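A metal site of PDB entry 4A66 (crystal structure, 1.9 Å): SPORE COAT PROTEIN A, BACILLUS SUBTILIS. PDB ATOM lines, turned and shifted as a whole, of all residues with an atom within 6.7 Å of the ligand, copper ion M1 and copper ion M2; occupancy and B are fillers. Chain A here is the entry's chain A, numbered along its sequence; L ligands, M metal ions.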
ATOM      1  N   HIS A 105       6.105 -25.218  -5.592  1.00  0.00           N
ATOM      2  CA  HIS A 105       6.498 -25.560  -6.949  1.00  0.00           C
ATOM      3  C   HIS A 105       7.328 -26.831  -6.902  1.00  0.00           C
ATOM      4  O   HIS A 105       8.341 -26.894  -6.184  1.00  0.00           O
ATOM      5  CB  HIS A 105       7.350 -24.410  -7.531  1.00  0.00           C
ATOM      6  CG  HIS A 105       7.986 -24.745  -8.839  1.00  0.00           C
ATOM      7  ND1 HIS A 105       7.260 -25.086  -9.958  1.00  0.00           N
ATOM      8  CD2 HIS A 105       9.286 -24.764  -9.219  1.00  0.00           C
ATOM      9  CE1 HIS A 105       8.083 -25.298 -10.974  1.00  0.00           C
ATOM     10  NE2 HIS A 105       9.316 -25.114 -10.532  1.00  0.00           N
ATOM     11  N   LEU A 106       6.862 -27.859  -7.625  1.00  0.00           N
ATOM     12  CA  LEU A 106       7.655 -29.077  -7.837  1.00  0.00           C
ATOM     13  C   LEU A 106       8.597 -28.790  -8.993  1.00  0.00           C
ATOM     14  O   LEU A 106       8.211 -28.847 -10.170  1.00  0.00           O
ATOM     15  CB  LEU A 106       6.765 -30.302  -8.154  1.00  0.00           C
ATOM     16  CG  LEU A 106       7.566 -31.629  -8.347  1.00  0.00           C
ATOM     17  CD1 LEU A 106       8.464 -31.948  -7.075  1.00  0.00           C
ATOM     18  CD2 LEU A 106       6.598 -32.770  -8.608  1.00  0.00           C
ATOM     19  N   HIS A 107       9.832 -28.431  -8.648  1.00  0.00           N
ATOM     20  CA  HIS A 107      10.848 -28.044  -9.622  1.00  0.00           C
ATOM     21  C   HIS A 107      11.293 -29.258 -10.453  1.00  0.00           C
ATOM     22  O   HIS A 107      11.786 -30.234  -9.900  1.00  0.00           O
ATOM     23  CB  HIS A 107      12.058 -27.469  -8.895  1.00  0.00           C
ATOM     24  CG  HIS A 107      13.120 -26.975  -9.809  1.00  0.00           C
ATOM     25  ND1 HIS A 107      13.489 -25.648  -9.867  1.00  0.00           N
ATOM     26  CD2 HIS A 107      13.857 -27.613 -10.763  1.00  0.00           C
ATOM     27  CE1 HIS A 107      14.444 -25.499 -10.773  1.00  0.00           C
ATOM     28  NE2 HIS A 107      14.667 -26.666 -11.350  1.00  0.00           N
ATOM     29  N   GLY A 108      11.144 -29.159 -11.767  1.00  0.00           N
ATOM     30  CA  GLY A 108      11.357 -30.295 -12.664  1.00  0.00           C
ATOM     31  C   GLY A 108      10.106 -31.159 -12.860  1.00  0.00           C
ATOM     32  O   GLY A 108      10.127 -32.058 -13.686  1.00  0.00           O
ATOM     33  N   GLY A 117       2.529 -24.814  -9.341  1.00  0.00           N
ATOM     34  CA  GLY A 117       2.980 -23.816  -8.354  1.00  0.00           C
ATOM     35  C   GLY A 117       3.323 -22.479  -9.013  1.00  0.00           C
ATOM     36  O   GLY A 117       4.377 -21.890  -8.785  1.00  0.00           O
ATOM     37  N   PRO A 119       3.526 -18.628  -9.729  1.00  0.00           N
ATOM     38  CA  PRO A 119       3.799 -17.617  -8.713  1.00  0.00           C
ATOM     39  C   PRO A 119       2.541 -16.826  -8.311  1.00  0.00           C
ATOM     40  O   PRO A 119       2.479 -16.338  -7.198  1.00  0.00           O
ATOM     41  CB  PRO A 119       4.828 -16.677  -9.354  1.00  0.00           C
ATOM     42  CG  PRO A 119       5.314 -17.388 -10.615  1.00  0.00           C
ATOM     43  CD  PRO A 119       4.351 -18.466 -10.946  1.00  0.00           C
ATOM     44  N   TRP A 151      13.024 -31.292  -6.742  1.00  0.00           N
ATOM     45  CA  TRP A 151      12.946 -30.721  -5.401  1.00  0.00           C
ATOM     46  C   TRP A 151      11.740 -29.789  -5.397  1.00  0.00           C
ATOM     47  O   TRP A 151      11.222 -29.441  -6.455  1.00  0.00           O
ATOM     48  CB  TRP A 151      14.264 -30.031  -4.989  1.00  0.00           C
ATOM     49  CG  TRP A 151      14.692 -28.763  -5.753  1.00  0.00           C
ATOM     50  CD1 TRP A 151      15.041 -28.675  -7.093  1.00  0.00           C
ATOM     51  CD2 TRP A 151      14.907 -27.460  -5.188  1.00  0.00           C
ATOM     52  NE1 TRP A 151      15.434 -27.371  -7.381  1.00  0.00           N
ATOM     53  CE2 TRP A 151      15.357 -26.610  -6.246  1.00  0.00           C
ATOM     54  CE3 TRP A 151      14.753 -26.916  -3.898  1.00  0.00           C
ATOM     55  CZ2 TRP A 151      15.653 -25.257  -6.047  1.00  0.00           C
ATOM     56  CZ3 TRP A 151      15.058 -25.581  -3.689  1.00  0.00           C
ATOM     57  CH2 TRP A 151      15.488 -24.748  -4.760  1.00  0.00           C
ATOM     58  N   HIS A 153       9.806 -26.300  -3.562  1.00  0.00           N
ATOM     59  CA  HIS A 153      10.098 -25.077  -2.851  1.00  0.00           C
ATOM     60  C   HIS A 153       8.991 -24.047  -3.103  1.00  0.00           C
ATOM     61  O   HIS A 153       8.203 -24.170  -4.077  1.00  0.00           O
ATOM     62  CB  HIS A 153      11.476 -24.519  -3.254  1.00  0.00           C
ATOM     63  CG  HIS A 153      11.602 -24.156  -4.705  1.00  0.00           C
ATOM     64  ND1 HIS A 153      11.179 -22.939  -5.208  1.00  0.00           N
ATOM     65  CD2 HIS A 153      12.137 -24.836  -5.745  1.00  0.00           C
ATOM     66  CE1 HIS A 153      11.438 -22.896  -6.509  1.00  0.00           C
ATOM     67  NE2 HIS A 153      12.026 -24.032  -6.854  1.00  0.00           N
ATOM     68  N   ASP A 154       8.907 -23.064  -2.203  1.00  0.00           N
ATOM     69  CA  ASP A 154       7.929 -21.988  -2.376  1.00  0.00           C
ATOM     70  C   ASP A 154       8.248 -21.196  -3.651  1.00  0.00           C
ATOM     71  O   ASP A 154       9.413 -21.055  -4.034  1.00  0.00           O
ATOM     72  CB  ASP A 154       7.966 -21.026  -1.184  1.00  0.00           C
ATOM     73  CG  ASP A 154       6.775 -20.085  -1.215  1.00  0.00           C
ATOM     74  OD1 ASP A 154       5.659 -20.555  -0.923  1.00  0.00           O
ATOM     75  OD2 ASP A 154       6.966 -18.943  -1.634  1.00  0.00           O
ATOM     76  N   HIS A 155       7.203 -20.660  -4.268  1.00  0.00           N
ATOM     77  CA  HIS A 155       7.355 -19.925  -5.506  1.00  0.00           C
ATOM     78  C   HIS A 155       6.443 -18.666  -5.525  1.00  0.00           C
ATOM     79  O   HIS A 155       6.123 -18.159  -6.600  1.00  0.00           O
ATOM     80  CB  HIS A 155       7.003 -20.832  -6.696  1.00  0.00           C
ATOM     81  CG  HIS A 155       7.775 -20.549  -7.947  1.00  0.00           C
ATOM     82  ND1 HIS A 155       7.864 -19.295  -8.514  1.00  0.00           N
ATOM     83  CD2 HIS A 155       8.524 -21.371  -8.745  1.00  0.00           C
ATOM     84  CE1 HIS A 155       8.617 -19.350  -9.607  1.00  0.00           C
ATOM     85  NE2 HIS A 155       9.016 -20.601  -9.784  1.00  0.00           N
ATOM     86  N   THR A 160       9.489 -15.182  -3.152  1.00  0.00           N
ATOM     87  CA  THR A 160      10.250 -16.446  -3.301  1.00  0.00           C
ATOM     88  C   THR A 160      11.575 -16.446  -2.533  1.00  0.00           C
ATOM     89  O   THR A 160      11.871 -17.400  -1.800  1.00  0.00           O
ATOM     90  CB  THR A 160      10.375 -16.798  -4.798  1.00  0.00           C
ATOM     91  OG1 THR A 160       9.036 -17.007  -5.293  1.00  0.00           O
ATOM     92  CG2 THR A 160      11.151 -18.094  -5.017  1.00  0.00           C
ATOM     93  N   ALA A 297      19.470 -24.339  -8.023  1.00  0.00           N
ATOM     94  CA  ALA A 297      18.465 -25.264  -8.600  1.00  0.00           C
ATOM     95  C   ALA A 297      18.998 -26.397  -9.472  1.00  0.00           C
ATOM     96  O   ALA A 297      18.254 -27.310  -9.789  1.00  0.00           O
ATOM     97  CB  ALA A 297      17.323 -24.504  -9.298  1.00  0.00           C
ATOM     98  N   HIS A 422      16.087 -21.135 -15.912  1.00  0.00           N
ATOM     99  CA  HIS A 422      15.256 -22.282 -15.679  1.00  0.00           C
ATOM    100  C   HIS A 422      13.939 -22.186 -16.451  1.00  0.00           C
ATOM    101  O   HIS A 422      13.295 -21.122 -16.463  1.00  0.00           O
ATOM    102  CB  HIS A 422      15.007 -22.430 -14.167  1.00  0.00           C
ATOM    103  CG  HIS A 422      13.998 -23.480 -13.816  1.00  0.00           C
ATOM    104  ND1 HIS A 422      14.129 -24.797 -14.192  1.00  0.00           N
ATOM    105  CD2 HIS A 422      12.854 -23.398 -13.106  1.00  0.00           C
ATOM    106  CE1 HIS A 422      13.093 -25.486 -13.734  1.00  0.00           C
ATOM    107  NE2 HIS A 422      12.307 -24.653 -13.073  1.00  0.00           N
ATOM    108  N   LEU A 423      13.543 -23.281 -17.104  1.00  0.00           N
ATOM    109  CA  LEU A 423      12.230 -23.352 -17.752  1.00  0.00           C
ATOM    110  C   LEU A 423      11.375 -24.320 -16.955  1.00  0.00           C
ATOM    111  O   LEU A 423      11.805 -25.418 -16.663  1.00  0.00           O
ATOM    112  CB  LEU A 423      12.353 -23.857 -19.202  1.00  0.00           C
ATOM    113  CG  LEU A 423      12.697 -22.826 -20.313  1.00  0.00           C
ATOM    114  CD1 LEU A 423      14.081 -22.211 -20.060  1.00  0.00           C
ATOM    115  CD2 LEU A 423      12.606 -23.501 -21.731  1.00  0.00           C
ATOM    116  N   HIS A 424      10.153 -23.929 -16.599  1.00  0.00           N
ATOM    117  CA  HIS A 424       9.237 -24.880 -15.958  1.00  0.00           C
ATOM    118  C   HIS A 424       8.795 -25.925 -16.965  1.00  0.00           C
ATOM    119  O   HIS A 424       8.983 -25.737 -18.168  1.00  0.00           O
ATOM    120  CB  HIS A 424       7.984 -24.153 -15.435  1.00  0.00           C
ATOM    121  CG  HIS A 424       8.225 -23.357 -14.200  1.00  0.00           C
ATOM    122  ND1 HIS A 424       7.202 -22.998 -13.343  1.00  0.00           N
ATOM    123  CD2 HIS A 424       9.368 -22.864 -13.646  1.00  0.00           C
ATOM    124  CE1 HIS A 424       7.699 -22.284 -12.344  1.00  0.00           C
ATOM    125  NE2 HIS A 424       9.012 -22.185 -12.496  1.00  0.00           N
ATOM    126  N   THR A 466      17.798 -26.329 -15.601  1.00  0.00           N
ATOM    127  CA  THR A 466      18.365 -25.105 -15.086  1.00  0.00           C
ATOM    128  C   THR A 466      19.800 -25.027 -15.617  1.00  0.00           C
ATOM    129  O   THR A 466      20.561 -25.957 -15.441  1.00  0.00           O
ATOM    130  CB  THR A 466      18.357 -25.081 -13.537  1.00  0.00           C
ATOM    131  OG1 THR A 466      17.017 -25.331 -13.057  1.00  0.00           O
ATOM    132  CG2 THR A 466      18.853 -23.733 -13.008  1.00  0.00           C
ATOM    133  N   VAL A 489       6.182 -20.841 -16.750  1.00  0.00           N
ATOM    134  CA  VAL A 489       7.098 -19.748 -16.412  1.00  0.00           C
ATOM    135  C   VAL A 489       8.492 -20.089 -16.916  1.00  0.00           C
ATOM    136  O   VAL A 489       8.817 -21.255 -17.046  1.00  0.00           O
ATOM    137  CB  VAL A 489       7.214 -19.557 -14.844  1.00  0.00           C
ATOM    138  CG1 VAL A 489       8.139 -18.341 -14.503  1.00  0.00           C
ATOM    139  CG2 VAL A 489       5.831 -19.337 -14.177  1.00  0.00           C
ATOM    140  N   TRP A 490       9.323 -19.076 -17.218  1.00  0.00           N
ATOM    141  CA  TRP A 490      10.760 -19.298 -17.314  1.00  0.00           C
ATOM    142  C   TRP A 490      11.428 -18.121 -16.622  1.00  0.00           C
ATOM    143  O   TRP A 490      10.876 -17.008 -16.638  1.00  0.00           O
ATOM    144  CB  TRP A 490      11.212 -19.472 -18.780  1.00  0.00           C
ATOM    145  CG  TRP A 490      11.235 -18.188 -19.602  1.00  0.00           C
ATOM    146  CD1 TRP A 490      10.153 -17.508 -20.128  1.00  0.00           C
ATOM    147  CD2 TRP A 490      12.397 -17.469 -19.999  1.00  0.00           C
ATOM    148  NE1 TRP A 490      10.592 -16.366 -20.810  1.00  0.00           N
ATOM    149  CE2 TRP A 490      11.960 -16.335 -20.754  1.00  0.00           C
ATOM    150  CE3 TRP A 490      13.773 -17.652 -19.785  1.00  0.00           C
ATOM    151  CZ2 TRP A 490      12.863 -15.425 -21.300  1.00  0.00           C
ATOM    152  CZ3 TRP A 490      14.670 -16.735 -20.331  1.00  0.00           C
ATOM    153  CH2 TRP A 490      14.204 -15.636 -21.086  1.00  0.00           C
ATOM    154  N   HIS A 491      12.557 -18.355 -15.990  1.00  0.00           N
ATOM    155  CA  HIS A 491      13.135 -17.350 -15.092  1.00  0.00           C
ATOM    156  C   HIS A 491      14.585 -17.667 -14.726  1.00  0.00           C
ATOM    157  O   HIS A 491      15.050 -18.815 -14.914  1.00  0.00           O
ATOM    158  CB  HIS A 491      12.301 -17.203 -13.796  1.00  0.00           C
ATOM    159  CG  HIS A 491      12.241 -18.435 -12.920  1.00  0.00           C
ATOM    160  ND1 HIS A 491      13.036 -18.592 -11.794  1.00  0.00           N
ATOM    161  CD2 HIS A 491      11.438 -19.517 -12.972  1.00  0.00           C
ATOM    162  CE1 HIS A 491      12.735 -19.746 -11.213  1.00  0.00           C
ATOM    163  NE2 HIS A 491      11.734 -20.301 -11.880  1.00  0.00           N
ATOM    164  N   CYS A 492      15.287 -16.659 -14.245  1.00  0.00           N
ATOM    165  CA  CYS A 492      16.562 -16.875 -13.567  1.00  0.00           C
ATOM    166  C   CYS A 492      16.279 -17.448 -12.184  1.00  0.00           C
ATOM    167  O   CYS A 492      15.362 -16.993 -11.524  1.00  0.00           O
ATOM    168  CB  CYS A 492      17.322 -15.575 -13.420  1.00  0.00           C
ATOM    169  SG  CYS A 492      18.824 -15.780 -12.497  1.00  0.00           S
ATOM    170  N   HIS A 493      17.064 -18.429 -11.754  1.00  0.00           N
ATOM    171  CA  HIS A 493      16.813 -19.100 -10.473  1.00  0.00           C
ATOM    172  C   HIS A 493      17.712 -18.540  -9.345  1.00  0.00           C
ATOM    173  O   HIS A 493      17.794 -19.124  -8.257  1.00  0.00           O
ATOM    174  CB  HIS A 493      16.936 -20.649 -10.601  1.00  0.00           C
ATOM    175  CG  HIS A 493      15.954 -21.405  -9.734  1.00  0.00           C
ATOM    176  ND1 HIS A 493      16.009 -21.367  -8.345  1.00  0.00           N
ATOM    177  CD2 HIS A 493      14.906 -22.215 -10.041  1.00  0.00           C
ATOM    178  CE1 HIS A 493      15.025 -22.114  -7.846  1.00  0.00           C
ATOM    179  NE2 HIS A 493      14.343 -22.643  -8.851  1.00  0.00           N
ATOM    180  N   LEU A 495      17.209 -16.190  -6.755  1.00  0.00           N
ATOM    181  CA  LEU A 495      15.905 -15.790  -6.242  1.00  0.00           C
ATOM    182  C   LEU A 495      15.799 -14.276  -6.093  1.00  0.00           C
ATOM    183  O   LEU A 495      14.736 -13.712  -6.318  1.00  0.00           O
ATOM    184  CB  LEU A 495      15.597 -16.518  -4.934  1.00  0.00           C
ATOM    185  CG  LEU A 495      15.646 -18.047  -5.043  1.00  0.00           C
ATOM    186  CD1 LEU A 495      15.087 -18.643  -3.728  1.00  0.00           C
ATOM    187  CD2 LEU A 495      14.813 -18.560  -6.243  1.00  0.00           C
ATOM    188  N   GLU A 498      15.030 -13.349  -9.679  1.00  0.00           N
ATOM    189  CA  GLU A 498      13.662 -13.821  -9.920  1.00  0.00           C
ATOM    190  C   GLU A 498      12.569 -12.873  -9.393  1.00  0.00           C
ATOM    191  O   GLU A 498      11.566 -12.580 -10.090  1.00  0.00           O
ATOM    192  CB  GLU A 498      13.508 -15.213  -9.296  1.00  0.00           C
ATOM    193  CG  GLU A 498      12.136 -15.794  -9.411  1.00  0.00           C
ATOM    194  CD  GLU A 498      12.083 -17.233  -8.946  1.00  0.00           C
ATOM    195  OE1 GLU A 498      13.145 -17.903  -8.896  1.00  0.00           O
ATOM    196  OE2 GLU A 498      10.974 -17.684  -8.645  1.00  0.00           O
ATOM    197  N   MET A 503      11.725 -12.939 -14.499  1.00  0.00           N
ATOM    198  CA  MET A 503      10.795 -14.036 -14.586  1.00  0.00           C
ATOM    199  C   MET A 503       9.700 -13.658 -15.546  1.00  0.00           C
ATOM    200  O   MET A 503       9.163 -12.564 -15.448  1.00  0.00           O
ATOM    201  CB  MET A 503      10.179 -14.298 -13.195  1.00  0.00           C
ATOM    202  CG  MET A 503       9.193 -15.482 -13.150  1.00  0.00           C
ATOM    203  SD  MET A 503       8.678 -15.976 -11.475  1.00  0.00           S
ATOM    204  CE  MET A 503       7.534 -14.660 -10.994  1.00  0.00           C
HETATM  205  O1  LIG L   1      11.559 -21.817  -9.494  1.00  0.00           O
HETATM  206  O2  LIG L   1      11.570 -23.108 -10.105  1.00  0.00           O
HETATM  207 CU    CU M   1      10.261 -21.488 -11.114  1.00  0.00          CU
HETATM  208 CU    CU M   2      13.003 -24.177  -8.615  1.00  0.00          CU
HETATM  209 CU    CU M   3      10.786 -24.980 -11.861  1.00  0.00          CU
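The backbone NH of His 424 is in hydrogen-bond range of the backbone carbonyl oxygen of Val 489, 3.0 Å away. A ring nitrogen (NE2) of His 107 sits close to a ring nitrogen (ND1) of His 422. O of Trp 151 lies within hydrogen-bond range of N of His 107, 2.8 Å away. The side-chain hydroxyl (OG1) of Thr 466 is in hydrogen-bond range of a ring nitrogen (NE2) of His 107, 3.2 Å away. The backbone carbonyl oxygen (O) of His 153 sits at hydrogen-bond distance from the backbone NH (N) of His 105 (2.8 Å). The backbone carbonyl oxygen (O) of His 155 lies close to the side-chain hydroxyl (OG1) of Thr 160, 3.4 Å away. OE1 of Glu 498 is in hydrogen-bond range of ND1 of His 491 (3.0 Å). A ring nitrogen (ND1) of His 422 is in hydrogen-bond range of the side-chain hydroxyl of Thr 466 (3.1 Å).
A ring nitrogen (NE2) of His 105 lies close to an oxygen (O2) of the ligand, at 3.0 Å. A ring nitrogen (NE2) of His 422 lies close to an oxygen (O2) of the ligand, at 3.4 Å. Hydrophobic or aromatic side chains that line the ligand: His 105, His 107, His 153, His 155, His 422, His 491 and His 493. Within 4 Å of the ligand: His 105, His 107, His 153, His 155, His 422, His 424, His 491 and His 493. The nearest printed residue that does not touch the ligand is Glu 498 (4.3 Å).
His 105 touches copper ion M1 (NE2 to CU, 3.8 Å). CD2 of His 422 touches copper ion M1 (3.8 Å). Five residues have an atom within 4 Å of copper ion M1: His 105, His 155, His 422, His 424 and His 491.
CD2 of His 105 touches copper ion M2, at 3.8 Å. Trp 151 touches copper ion M2 (CZ2 to CU, 3.8 Å). Within 4 Å of copper ion M2: His 105, His 107, Trp 151, His 153 and His 493.
Copper ion M1 is bound by a ring nitrogen (NE2) of His 424, a ring nitrogen (NE2) of His 155, a ring nitrogen (NE2) of His 491 and an oxygen (O1) of the ligand.
ND1 of His 107 is bound to copper ion M2 (2.0 Å). NE2 of His 153 binds copper ion M2, at 2.0 Å. A ring nitrogen (NE2) of His 493 binds copper ion M2 (2.1 Å). An oxygen (O2) of the ligand is bound to copper ion M2, at 2.3 Å. Copper ion M2 has four donor atoms within binding distance.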
